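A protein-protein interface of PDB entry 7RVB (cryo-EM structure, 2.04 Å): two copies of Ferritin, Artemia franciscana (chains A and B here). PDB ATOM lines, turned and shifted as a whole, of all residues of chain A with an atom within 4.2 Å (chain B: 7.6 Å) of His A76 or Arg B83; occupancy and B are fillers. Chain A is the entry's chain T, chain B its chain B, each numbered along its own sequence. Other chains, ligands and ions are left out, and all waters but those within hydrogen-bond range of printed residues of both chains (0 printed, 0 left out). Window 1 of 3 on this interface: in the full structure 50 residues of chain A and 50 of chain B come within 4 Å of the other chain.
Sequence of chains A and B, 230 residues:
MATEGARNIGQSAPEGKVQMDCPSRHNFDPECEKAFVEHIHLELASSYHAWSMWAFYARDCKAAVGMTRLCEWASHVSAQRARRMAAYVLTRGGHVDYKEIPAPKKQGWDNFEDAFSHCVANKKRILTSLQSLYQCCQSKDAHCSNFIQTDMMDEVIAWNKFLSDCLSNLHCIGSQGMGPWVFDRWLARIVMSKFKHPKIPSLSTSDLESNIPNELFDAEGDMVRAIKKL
A ring nitrogen (NE2) of His A197 sits close to a ring nitrogen (NE2) of His A76.
Positions printed for both chains: 76, 77, 78, 79, 80 and 197. Of the 6 pairs that touch across the chains among the printed residues, none has its exchanged pair printed and touching as well.
Trp A51 touches Arg B83. CE3 of Trp A51 touches OH of Tyr B98, at 3.3 Å. Val A77 touches Pro B201.
The backbone carbonyl oxygen of Pro B201 lies within hydrogen-bond range of the indole nitrogen of Trp A73 (2.9 Å). The backbone carbonyl oxygen (O) of Ile B200 is in hydrogen-bond range of the side-chain amide nitrogen (NE2) of Gln A80. The guanidinium group of Arg B83 lies within hydrogen-bond range of a ring nitrogen (NE2) of His A76, at 3.0 Å.
Printed residues of chain B within 4 Å of Trp A51: Arg B83 (3.7 Å) and Tyr B98 (3.3 Å). No residue of chain B comes within 4 Å of Ser A75. His A76 touches one residue of chain B. His A197 touches none of the printed residues of chain B. Of chain A, only Trp A51 (3.7 Å) and His A76 (3.0 Å) come within 4 Å of Arg B83. Ala B86 touches none of the printed residues of chain A. Of the printed residues of chain A, Pro B201 touches Trp A73 (2.9 Å) and Val A77 (3.96 Å). The nearest residue of chain B that does not touch His A76 is Ile B200 (4.2 Å). The nearest printed residue of chain A that does not touch Arg B83 is His A197 (4.2 Å).
Of the 12 printed residues of chain A, 5 touch a printed residue of chain B. Along chain A the printed residues that touch a printed residue of chain B span positions 51 to 80. Of the 22 printed residues of chain B, 4 touch a printed residue of chain A. Printed residues of chain B that touch a printed residue of chain A: Arg B83, Tyr B98, Ile B200 and Pro B201. Hydrophobic or aromatic side chains of chain B within 4 Å of the printed part of chain A: Tyr B98 and Ile B200. Among the printed residues, 6 pairs touch across the chains.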
ATOM      1  N   TRP A  51      22.925   8.479 -12.293  1.00  0.00           N
ATOM      2  CA  TRP A  51      22.127   7.271 -12.095  1.00  0.00           C
ATOM      3  C   TRP A  51      21.391   6.870 -13.366  1.00  0.00           C
ATOM      4  O   TRP A  51      21.268   5.678 -13.670  1.00  0.00           O
ATOM      5  CB  TRP A  51      21.118   7.487 -10.968  1.00  0.00           C
ATOM      6  CG  TRP A  51      21.517   6.911  -9.661  1.00  0.00           C
ATOM      7  CD1 TRP A  51      22.674   7.137  -8.988  1.00  0.00           C
ATOM      8  CD2 TRP A  51      20.760   5.996  -8.866  1.00  0.00           C
ATOM      9  NE1 TRP A  51      22.685   6.427  -7.814  1.00  0.00           N
ATOM     10  CE2 TRP A  51      21.520   5.715  -7.717  1.00  0.00           C
ATOM     11  CE3 TRP A  51      19.511   5.389  -9.014  1.00  0.00           C
ATOM     12  CZ2 TRP A  51      21.074   4.854  -6.721  1.00  0.00           C
ATOM     13  CZ3 TRP A  51      19.071   4.535  -8.025  1.00  0.00           C
ATOM     14  CH2 TRP A  51      19.849   4.275  -6.894  1.00  0.00           C
ATOM     15  N   GLU A  72      28.559   4.425 -12.182  1.00  0.00           N
ATOM     16  CA  GLU A  72      28.382   4.185 -10.752  1.00  0.00           C
ATOM     17  C   GLU A  72      29.431   4.935  -9.935  1.00  0.00           C
ATOM     18  O   GLU A  72      29.111   5.608  -8.937  1.00  0.00           O
ATOM     19  CB  GLU A  72      28.452   2.685 -10.478  1.00  0.00           C
ATOM     20  CG  GLU A  72      27.848   2.258  -9.166  1.00  0.00           C
ATOM     21  CD  GLU A  72      28.226   0.841  -8.792  1.00  0.00           C
ATOM     22  OE1 GLU A  72      28.093   0.485  -7.601  1.00  0.00           O
ATOM     23  OE2 GLU A  72      28.659   0.084  -9.686  1.00  0.00           O
ATOM     24  N   TRP A  73      30.693   4.850 -10.365  1.00  0.00           N
ATOM     25  CA  TRP A  73      31.764   5.554  -9.670  1.00  0.00           C
ATOM     26  C   TRP A  73      31.525   7.058  -9.668  1.00  0.00           C
ATOM     27  O   TRP A  73      31.707   7.724  -8.638  1.00  0.00           O
ATOM     28  CB  TRP A  73      33.101   5.216 -10.325  1.00  0.00           C
ATOM     29  CG  TRP A  73      34.298   5.703  -9.586  1.00  0.00           C
ATOM     30  CD1 TRP A  73      34.372   6.031  -8.269  1.00  0.00           C
ATOM     31  CD2 TRP A  73      35.604   5.914 -10.127  1.00  0.00           C
ATOM     32  NE1 TRP A  73      35.642   6.436  -7.953  1.00  0.00           N
ATOM     33  CE2 TRP A  73      36.419   6.373  -9.078  1.00  0.00           C
ATOM     34  CE3 TRP A  73      36.163   5.759 -11.397  1.00  0.00           C
ATOM     35  CZ2 TRP A  73      37.762   6.679  -9.259  1.00  0.00           C
ATOM     36  CZ3 TRP A  73      37.494   6.064 -11.574  1.00  0.00           C
ATOM     37  CH2 TRP A  73      38.280   6.518 -10.511  1.00  0.00           C
ATOM     38  N   ALA A  74      31.104   7.611 -10.808  1.00  0.00           N
ATOM     39  CA  ALA A  74      30.873   9.049 -10.895  1.00  0.00           C
ATOM     40  C   ALA A  74      29.763   9.495  -9.952  1.00  0.00           C
ATOM     41  O   ALA A  74      29.877  10.540  -9.296  1.00  0.00           O
ATOM     42  CB  ALA A  74      30.543   9.440 -12.333  1.00  0.00           C
ATOM     43  N   SER A  75      28.674   8.724  -9.877  1.00  0.00           N
ATOM     44  CA  SER A  75      27.582   9.104  -8.985  1.00  0.00           C
ATOM     45  C   SER A  75      28.037   9.117  -7.531  1.00  0.00           C
ATOM     46  O   SER A  75      27.719  10.051  -6.777  1.00  0.00           O
ATOM     47  CB  SER A  75      26.393   8.163  -9.172  1.00  0.00           C
ATOM     48  OG  SER A  75      26.596   6.944  -8.490  1.00  0.00           O
ATOM     49  N   HIS A  76      28.801   8.100  -7.120  1.00  0.00           N
ATOM     50  CA  HIS A  76      29.285   8.089  -5.741  1.00  0.00           C
ATOM     51  C   HIS A  76      30.215   9.268  -5.462  1.00  0.00           C
ATOM     52  O   HIS A  76      30.145   9.888  -4.390  1.00  0.00           O
ATOM     53  CB  HIS A  76      29.972   6.762  -5.433  1.00  0.00           C
ATOM     54  CG  HIS A  76      29.022   5.675  -5.045  1.00  0.00           C
ATOM     55  ND1 HIS A  76      28.352   5.667  -3.842  1.00  0.00           N
ATOM     56  CD2 HIS A  76      28.616   4.567  -5.708  1.00  0.00           C
ATOM     57  CE1 HIS A  76      27.581   4.598  -3.777  1.00  0.00           C
ATOM     58  NE2 HIS A  76      27.723   3.914  -4.896  1.00  0.00           N
ATOM     59  N   VAL A  77      31.084   9.603  -6.420  1.00  0.00           N
ATOM     60  CA  VAL A  77      32.003  10.725  -6.231  1.00  0.00           C
ATOM     61  C   VAL A  77      31.235  12.032  -6.054  1.00  0.00           C
ATOM     62  O   VAL A  77      31.553  12.845  -5.174  1.00  0.00           O
ATOM     63  CB  VAL A  77      32.994  10.803  -7.409  1.00  0.00           C
ATOM     64  CG1 VAL A  77      33.691  12.147  -7.434  1.00  0.00           C
ATOM     65  CG2 VAL A  77      34.009   9.684  -7.321  1.00  0.00           C
ATOM     66  N   SER A  78      30.215  12.255  -6.885  1.00  0.00           N
ATOM     67  CA  SER A  78      29.436  13.487  -6.775  1.00  0.00           C
ATOM     68  C   SER A  78      28.707  13.572  -5.437  1.00  0.00           C
ATOM     69  O   SER A  78      28.647  14.647  -4.818  1.00  0.00           O
ATOM     70  CB  SER A  78      28.446  13.584  -7.932  1.00  0.00           C
ATOM     71  OG  SER A  78      29.065  14.121  -9.082  1.00  0.00           O
ATOM     72  N   ALA A  79      28.141  12.453  -4.976  1.00  0.00           N
ATOM     73  CA  ALA A  79      27.476  12.466  -3.675  1.00  0.00           C
ATOM     74  C   ALA A  79      28.454  12.824  -2.560  1.00  0.00           C
ATOM     75  O   ALA A  79      28.128  13.616  -1.662  1.00  0.00           O
ATOM     76  CB  ALA A  79      26.822  11.113  -3.403  1.00  0.00           C
ATOM     77  N   GLN A  80      29.663  12.258  -2.608  1.00  0.00           N
ATOM     78  CA  GLN A  80      30.658  12.584  -1.591  1.00  0.00           C
ATOM     79  C   GLN A  80      31.029  14.063  -1.627  1.00  0.00           C
ATOM     80  O   GLN A  80      31.219  14.688  -0.577  1.00  0.00           O
ATOM     81  CB  GLN A  80      31.899  11.714  -1.769  1.00  0.00           C
ATOM     82  CG  GLN A  80      32.989  11.988  -0.755  1.00  0.00           C
ATOM     83  CD  GLN A  80      34.060  10.922  -0.743  1.00  0.00           C
ATOM     84  OE1 GLN A  80      34.037  10.016   0.087  1.00  0.00           O
ATOM     85  NE2 GLN A  80      35.006  11.023  -1.663  1.00  0.00           N
ATOM     86  N   PHE A 195      38.140   1.332  -8.046  1.00  0.00           N
ATOM     87  CA  PHE A 195      36.920   1.534  -7.281  1.00  0.00           C
ATOM     88  C   PHE A 195      36.157   0.230  -7.116  1.00  0.00           C
ATOM     89  O   PHE A 195      36.067  -0.576  -8.046  1.00  0.00           O
ATOM     90  CB  PHE A 195      36.022   2.578  -7.947  1.00  0.00           C
ATOM     91  CG  PHE A 195      34.668   2.701  -7.318  1.00  0.00           C
ATOM     92  CD1 PHE A 195      34.531   3.189  -6.033  1.00  0.00           C
ATOM     93  CD2 PHE A 195      33.532   2.339  -8.013  1.00  0.00           C
ATOM     94  CE1 PHE A 195      33.290   3.307  -5.452  1.00  0.00           C
ATOM     95  CE2 PHE A 195      32.288   2.457  -7.437  1.00  0.00           C
ATOM     96  CZ  PHE A 195      32.167   2.941  -6.155  1.00  0.00           C
ATOM     97  N   HIS A 197      32.571  -0.586  -4.721  1.00  0.00           N
ATOM     98  CA  HIS A 197      31.649  -0.130  -3.688  1.00  0.00           C
ATOM     99  C   HIS A 197      31.320  -1.265  -2.730  1.00  0.00           C
ATOM    100  O   HIS A 197      30.780  -2.288  -3.162  1.00  0.00           O
ATOM    101  CB  HIS A 197      30.369   0.412  -4.291  1.00  0.00           C
ATOM    102  CG  HIS A 197      29.490   1.094  -3.291  1.00  0.00           C
ATOM    103  ND1 HIS A 197      29.997   1.837  -2.247  1.00  0.00           N
ATOM    104  CD2 HIS A 197      28.144   1.131  -3.160  1.00  0.00           C
ATOM    105  CE1 HIS A 197      29.000   2.312  -1.521  1.00  0.00           C
ATOM    106  NE2 HIS A 197      27.865   1.897  -2.054  1.00  0.00           N
ATOM    107  N   ILE B  40      10.437   2.723  -6.461  1.00  0.00           N
ATOM    108  CA  ILE B  40      11.821   3.188  -6.517  1.00  0.00           C
ATOM    109  C   ILE B  40      11.892   4.668  -6.173  1.00  0.00           C
ATOM    110  O   ILE B  40      12.752   5.108  -5.397  1.00  0.00           O
ATOM    111  CB  ILE B  40      12.428   2.906  -7.903  1.00  0.00           C
ATOM    112  CG1 ILE B  40      12.742   1.423  -8.062  1.00  0.00           C
ATOM    113  CG2 ILE B  40      13.683   3.726  -8.114  1.00  0.00           C
ATOM    114  CD1 ILE B  40      13.033   1.018  -9.481  1.00  0.00           C
ATOM    115  N   GLU B  43      11.494   5.210  -2.444  1.00  0.00           N
ATOM    116  CA  GLU B  43      12.718   4.935  -1.691  1.00  0.00           C
ATOM    117  C   GLU B  43      13.734   6.061  -1.849  1.00  0.00           C
ATOM    118  O   GLU B  43      14.414   6.441  -0.885  1.00  0.00           O
ATOM    119  CB  GLU B  43      13.323   3.602  -2.128  1.00  0.00           C
ATOM    120  CG  GLU B  43      12.440   2.399  -1.858  1.00  0.00           C
ATOM    121  CD  GLU B  43      12.617   1.835  -0.461  1.00  0.00           C
ATOM    122  OE1 GLU B  43      13.370   2.429   0.334  1.00  0.00           O
ATOM    123  OE2 GLU B  43      11.996   0.796  -0.156  1.00  0.00           O
ATOM    124  N   LEU B  44      13.858   6.604  -3.064  1.00  0.00           N
ATOM    125  CA  LEU B  44      14.777   7.721  -3.273  1.00  0.00           C
ATOM    126  C   LEU B  44      14.369   8.936  -2.448  1.00  0.00           C
ATOM    127  O   LEU B  44      15.225   9.629  -1.883  1.00  0.00           O
ATOM    128  CB  LEU B  44      14.843   8.080  -4.757  1.00  0.00           C
ATOM    129  CG  LEU B  44      15.713   7.183  -5.634  1.00  0.00           C
ATOM    130  CD1 LEU B  44      15.576   7.574  -7.089  1.00  0.00           C
ATOM    131  CD2 LEU B  44      17.161   7.251  -5.198  1.00  0.00           C
ATOM    132  N   HIS B  76      22.062   5.927   3.714  1.00  0.00           N
ATOM    133  CA  HIS B  76      22.782   4.960   2.887  1.00  0.00           C
ATOM    134  C   HIS B  76      21.958   3.694   2.657  1.00  0.00           C
ATOM    135  O   HIS B  76      21.941   3.145   1.545  1.00  0.00           O
ATOM    136  CB  HIS B  76      24.133   4.629   3.515  1.00  0.00           C
ATOM    137  CG  HIS B  76      25.202   5.620   3.182  1.00  0.00           C
ATOM    138  ND1 HIS B  76      25.753   5.724   1.924  1.00  0.00           N
ATOM    139  CD2 HIS B  76      25.812   6.563   3.938  1.00  0.00           C
ATOM    140  CE1 HIS B  76      26.661   6.683   1.921  1.00  0.00           C
ATOM    141  NE2 HIS B  76      26.716   7.207   3.131  1.00  0.00           N
ATOM    142  N   VAL B  77      21.257   3.223   3.692  1.00  0.00           N
ATOM    143  CA  VAL B  77      20.438   2.019   3.550  1.00  0.00           C
ATOM    144  C   VAL B  77      19.337   2.232   2.514  1.00  0.00           C
ATOM    145  O   VAL B  77      19.084   1.366   1.664  1.00  0.00           O
ATOM    146  CB  VAL B  77      19.861   1.605   4.916  1.00  0.00           C
ATOM    147  CG1 VAL B  77      18.729   0.614   4.742  1.00  0.00           C
ATOM    148  CG2 VAL B  77      20.945   1.017   5.793  1.00  0.00           C
ATOM    149  N   SER B  78      18.665   3.384   2.569  1.00  0.00           N
ATOM    150  CA  SER B  78      17.596   3.655   1.610  1.00  0.00           C
ATOM    151  C   SER B  78      18.127   3.730   0.183  1.00  0.00           C
ATOM    152  O   SER B  78      17.494   3.219  -0.756  1.00  0.00           O
ATOM    153  CB  SER B  78      16.876   4.948   1.983  1.00  0.00           C
ATOM    154  OG  SER B  78      15.888   4.711   2.963  1.00  0.00           O
ATOM    155  N   ALA B  79      19.287   4.367  -0.007  1.00  0.00           N
ATOM    156  CA  ALA B  79      19.868   4.422  -1.346  1.00  0.00           C
ATOM    157  C   ALA B  79      20.171   3.023  -1.873  1.00  0.00           C
ATOM    158  O   ALA B  79      19.901   2.715  -3.045  1.00  0.00           O
ATOM    159  CB  ALA B  79      21.132   5.279  -1.338  1.00  0.00           C
ATOM    160  N   GLN B  80      20.722   2.158  -1.018  1.00  0.00           N
ATOM    161  CA  GLN B  80      21.006   0.792  -1.448  1.00  0.00           C
ATOM    162  C   GLN B  80      19.729   0.049  -1.827  1.00  0.00           C
ATOM    163  O   GLN B  80      19.714  -0.718  -2.797  1.00  0.00           O
ATOM    164  CB  GLN B  80      21.760   0.040  -0.353  1.00  0.00           C
ATOM    165  CG  GLN B  80      22.094  -1.392  -0.714  1.00  0.00           C
ATOM    166  CD  GLN B  80      23.100  -2.013   0.226  1.00  0.00           C
ATOM    167  OE1 GLN B  80      24.292  -2.058  -0.067  1.00  0.00           O
ATOM    168  NE2 GLN B  80      22.626  -2.498   1.363  1.00  0.00           N
ATOM    169  N   ARG B  81      18.648   0.257  -1.072  1.00  0.00           N
ATOM    170  CA  ARG B  81      17.387  -0.407  -1.399  1.00  0.00           C
ATOM    171  C   ARG B  81      16.860   0.033  -2.763  1.00  0.00           C
ATOM    172  O   ARG B  81      16.383  -0.796  -3.556  1.00  0.00           O
ATOM    173  CB  ARG B  81      16.349  -0.131  -0.314  1.00  0.00           C
ATOM    174  CG  ARG B  81      16.525  -0.971   0.933  1.00  0.00           C
ATOM    175  CD  ARG B  81      15.682  -0.443   2.077  1.00  0.00           C
ATOM    176  NE  ARG B  81      14.259  -0.507   1.778  1.00  0.00           N
ATOM    177  CZ  ARG B  81      13.530  -1.611   1.843  1.00  0.00           C
ATOM    178  NH1 ARG B  81      14.057  -2.766   2.211  1.00  0.00           N
ATOM    179  NH2 ARG B  81      12.239  -1.556   1.532  1.00  0.00           N
ATOM    180  N   ALA B  82      16.927   1.335  -3.050  1.00  0.00           N
ATOM    181  CA  ALA B  82      16.488   1.814  -4.359  1.00  0.00           C
ATOM    182  C   ALA B  82      17.322   1.197  -5.476  1.00  0.00           C
ATOM    183  O   ALA B  82      16.783   0.775  -6.513  1.00  0.00           O
ATOM    184  CB  ALA B  82      16.559   3.337  -4.415  1.00  0.00           C
ATOM    185  N   ARG B  83      18.639   1.126  -5.277  1.00  0.00           N
ATOM    186  CA  ARG B  83      19.502   0.505  -6.276  1.00  0.00           C
ATOM    187  C   ARG B  83      19.130  -0.956  -6.499  1.00  0.00           C
ATOM    188  O   ARG B  83      19.113  -1.434  -7.640  1.00  0.00           O
ATOM    189  CB  ARG B  83      20.963   0.627  -5.849  1.00  0.00           C
ATOM    190  CG  ARG B  83      21.963   0.141  -6.875  1.00  0.00           C
ATOM    191  CD  ARG B  83      23.351   0.689  -6.580  1.00  0.00           C
ATOM    192  NE  ARG B  83      23.414   1.313  -5.263  1.00  0.00           N
ATOM    193  CZ  ARG B  83      24.206   2.327  -4.947  1.00  0.00           C
ATOM    194  NH1 ARG B  83      25.032   2.863  -5.830  1.00  0.00           N
ATOM    195  NH2 ARG B  83      24.169   2.817  -3.711  1.00  0.00           N
ATOM    196  N   ARG B  84      18.834  -1.682  -5.419  1.00  0.00           N
ATOM    197  CA  ARG B  84      18.481  -3.093  -5.547  1.00  0.00           C
ATOM    198  C   ARG B  84      17.193  -3.281  -6.342  1.00  0.00           C
ATOM    199  O   ARG B  84      17.108  -4.171  -7.200  1.00  0.00           O
ATOM    200  CB  ARG B  84      18.354  -3.726  -4.164  1.00  0.00           C
ATOM    201  CG  ARG B  84      17.849  -5.152  -4.180  1.00  0.00           C
ATOM    202  CD  ARG B  84      18.380  -5.935  -2.999  1.00  0.00           C
ATOM    203  NE  ARG B  84      17.784  -5.500  -1.744  1.00  0.00           N
ATOM    204  CZ  ARG B  84      18.475  -5.125  -0.677  1.00  0.00           C
ATOM    205  NH1 ARG B  84      19.796  -5.129  -0.674  1.00  0.00           N
ATOM    206  NH2 ARG B  84      17.823  -4.736   0.413  1.00  0.00           N
ATOM    207  N   MET B  85      16.175  -2.460  -6.073  1.00  0.00           N
ATOM    208  CA  MET B  85      14.930  -2.601  -6.826  1.00  0.00           C
ATOM    209  C   MET B  85      15.134  -2.276  -8.304  1.00  0.00           C
ATOM    210  O   MET B  85      14.590  -2.964  -9.183  1.00  0.00           O
ATOM    211  CB  MET B  85      13.835  -1.723  -6.229  1.00  0.00           C
ATOM    212  CG  MET B  85      12.484  -1.924  -6.897  1.00  0.00           C
ATOM    213  SD  MET B  85      11.066  -1.524  -5.862  1.00  0.00           S
ATOM    214  CE  MET B  85      10.818  -3.071  -5.008  1.00  0.00           C
ATOM    215  N   ALA B  86      15.920  -1.236  -8.604  1.00  0.00           N
ATOM    216  CA  ALA B  86      16.199  -0.925 -10.003  1.00  0.00           C
ATOM    217  C   ALA B  86      16.935  -2.071 -10.688  1.00  0.00           C
ATOM    218  O   ALA B  86      16.643  -2.409 -11.844  1.00  0.00           O
ATOM    219  CB  ALA B  86      17.004   0.368 -10.106  1.00  0.00           C
ATOM    220  N   ALA B  87      17.893  -2.682  -9.989  1.00  0.00           N
ATOM    221  CA  ALA B  87      18.615  -3.814 -10.558  1.00  0.00           C
ATOM    222  C   ALA B  87      17.680  -4.981 -10.837  1.00  0.00           C
ATOM    223  O   ALA B  87      17.815  -5.660 -11.860  1.00  0.00           O
ATOM    224  CB  ALA B  87      19.743  -4.244  -9.624  1.00  0.00           C
ATOM    225  N   TYR B  88      16.731  -5.240  -9.934  1.00  0.00           N
ATOM    226  CA  TYR B  88      15.785  -6.322 -10.191  1.00  0.00           C
ATOM    227  C   TYR B  88      14.941  -6.034 -11.423  1.00  0.00           C
ATOM    228  O   TYR B  88      14.690  -6.932 -12.233  1.00  0.00           O
ATOM    229  CB  TYR B  88      14.875  -6.570  -8.992  1.00  0.00           C
ATOM    230  CG  TYR B  88      13.949  -7.740  -9.233  1.00  0.00           C
ATOM    231  CD1 TYR B  88      14.389  -9.041  -9.044  1.00  0.00           C
ATOM    232  CD2 TYR B  88      12.651  -7.551  -9.682  1.00  0.00           C
ATOM    233  CE1 TYR B  88      13.562 -10.113  -9.276  1.00  0.00           C
ATOM    234  CE2 TYR B  88      11.817  -8.620  -9.919  1.00  0.00           C
ATOM    235  CZ  TYR B  88      12.279  -9.900  -9.713  1.00  0.00           C
ATOM    236  OH  TYR B  88      11.459 -10.974  -9.944  1.00  0.00           O
ATOM    237  N   VAL B  89      14.481  -4.790 -11.578  1.00  0.00           N
ATOM    238  CA  VAL B  89      13.696  -4.457 -12.766  1.00  0.00           C
ATOM    239  C   VAL B  89      14.523  -4.675 -14.027  1.00  0.00           C
ATOM    240  O   VAL B  89      14.034  -5.224 -15.021  1.00  0.00           O
ATOM    241  CB  VAL B  89      13.159  -3.018 -12.683  1.00  0.00           C
ATOM    242  CG1 VAL B  89      12.715  -2.542 -14.052  1.00  0.00           C
ATOM    243  CG2 VAL B  89      12.006  -2.945 -11.713  1.00  0.00           C
ATOM    244  N   LEU B  90      15.791  -4.260 -14.006  1.00  0.00           N
ATOM    245  CA  LEU B  90      16.635  -4.433 -15.185  1.00  0.00           C
ATOM    246  C   LEU B  90      16.912  -5.903 -15.483  1.00  0.00           C
ATOM    247  O   LEU B  90      17.044  -6.279 -16.652  1.00  0.00           O
ATOM    248  CB  LEU B  90      17.948  -3.676 -15.011  1.00  0.00           C
ATOM    249  CG  LEU B  90      17.845  -2.154 -15.074  1.00  0.00           C
ATOM    250  CD1 LEU B  90      19.103  -1.518 -14.525  1.00  0.00           C
ATOM    251  CD2 LEU B  90      17.582  -1.695 -16.491  1.00  0.00           C
ATOM    252  N   TYR B  98      13.396   7.831 -14.721  1.00  0.00           N
ATOM    253  CA  TYR B  98      13.552   8.627 -13.516  1.00  0.00           C
ATOM    254  C   TYR B  98      12.860   9.972 -13.672  1.00  0.00           C
ATOM    255  O   TYR B  98      12.814  10.545 -14.762  1.00  0.00           O
ATOM    256  CB  TYR B  98      15.029   8.835 -13.186  1.00  0.00           C
ATOM    257  CG  TYR B  98      15.707   7.585 -12.690  1.00  0.00           C
ATOM    258  CD1 TYR B  98      15.506   7.136 -11.396  1.00  0.00           C
ATOM    259  CD2 TYR B  98      16.539   6.848 -13.516  1.00  0.00           C
ATOM    260  CE1 TYR B  98      16.118   5.995 -10.935  1.00  0.00           C
ATOM    261  CE2 TYR B  98      17.156   5.704 -13.065  1.00  0.00           C
ATOM    262  CZ  TYR B  98      16.942   5.282 -11.773  1.00  0.00           C
ATOM    263  OH  TYR B  98      17.552   4.143 -11.312  1.00  0.00           O
ATOM    264  N   HIS B 197      31.077   4.283   7.257  1.00  0.00           N
ATOM    265  CA  HIS B 197      31.114   4.523   5.818  1.00  0.00           C
ATOM    266  C   HIS B 197      32.543   4.752   5.347  1.00  0.00           C
ATOM    267  O   HIS B 197      33.194   5.693   5.814  1.00  0.00           O
ATOM    268  CB  HIS B 197      30.259   5.713   5.434  1.00  0.00           C
ATOM    269  CG  HIS B 197      30.087   5.861   3.956  1.00  0.00           C
ATOM    270  ND1 HIS B 197      29.983   4.778   3.112  1.00  0.00           N
ATOM    271  CD2 HIS B 197      30.024   6.960   3.167  1.00  0.00           C
ATOM    272  CE1 HIS B 197      29.851   5.202   1.868  1.00  0.00           C
ATOM    273  NE2 HIS B 197      29.874   6.522   1.874  1.00  0.00           N
ATOM    274  N   ILE B 200      35.302   7.260  -0.568  1.00  0.00           N
ATOM    275  CA  ILE B 200      35.239   6.948  -1.991  1.00  0.00           C
ATOM    276  C   ILE B 200      36.523   7.457  -2.642  1.00  0.00           C
ATOM    277  O   ILE B 200      36.804   8.661  -2.559  1.00  0.00           O
ATOM    278  CB  ILE B 200      34.007   7.578  -2.651  1.00  0.00           C
ATOM    279  CG1 ILE B 200      32.737   7.217  -1.878  1.00  0.00           C
ATOM    280  CG2 ILE B 200      33.898   7.144  -4.101  1.00  0.00           C
ATOM    281  CD1 ILE B 200      32.298   5.786  -2.047  1.00  0.00           C
ATOM    282  N   PRO B 201      37.317   6.599  -3.274  1.00  0.00           N
ATOM    283  CA  PRO B 201      38.523   7.073  -3.959  1.00  0.00           C
ATOM    284  C   PRO B 201      38.181   7.901  -5.189  1.00  0.00           C
ATOM    285  O   PRO B 201      37.114   7.766  -5.789  1.00  0.00           O
ATOM    286  CB  PRO B 201      39.245   5.780  -4.345  1.00  0.00           C
ATOM    287  CG  PRO B 201      38.173   4.763  -4.416  1.00  0.00           C
ATOM    288  CD  PRO B 201      37.154   5.141  -3.386  1.00  0.00           C
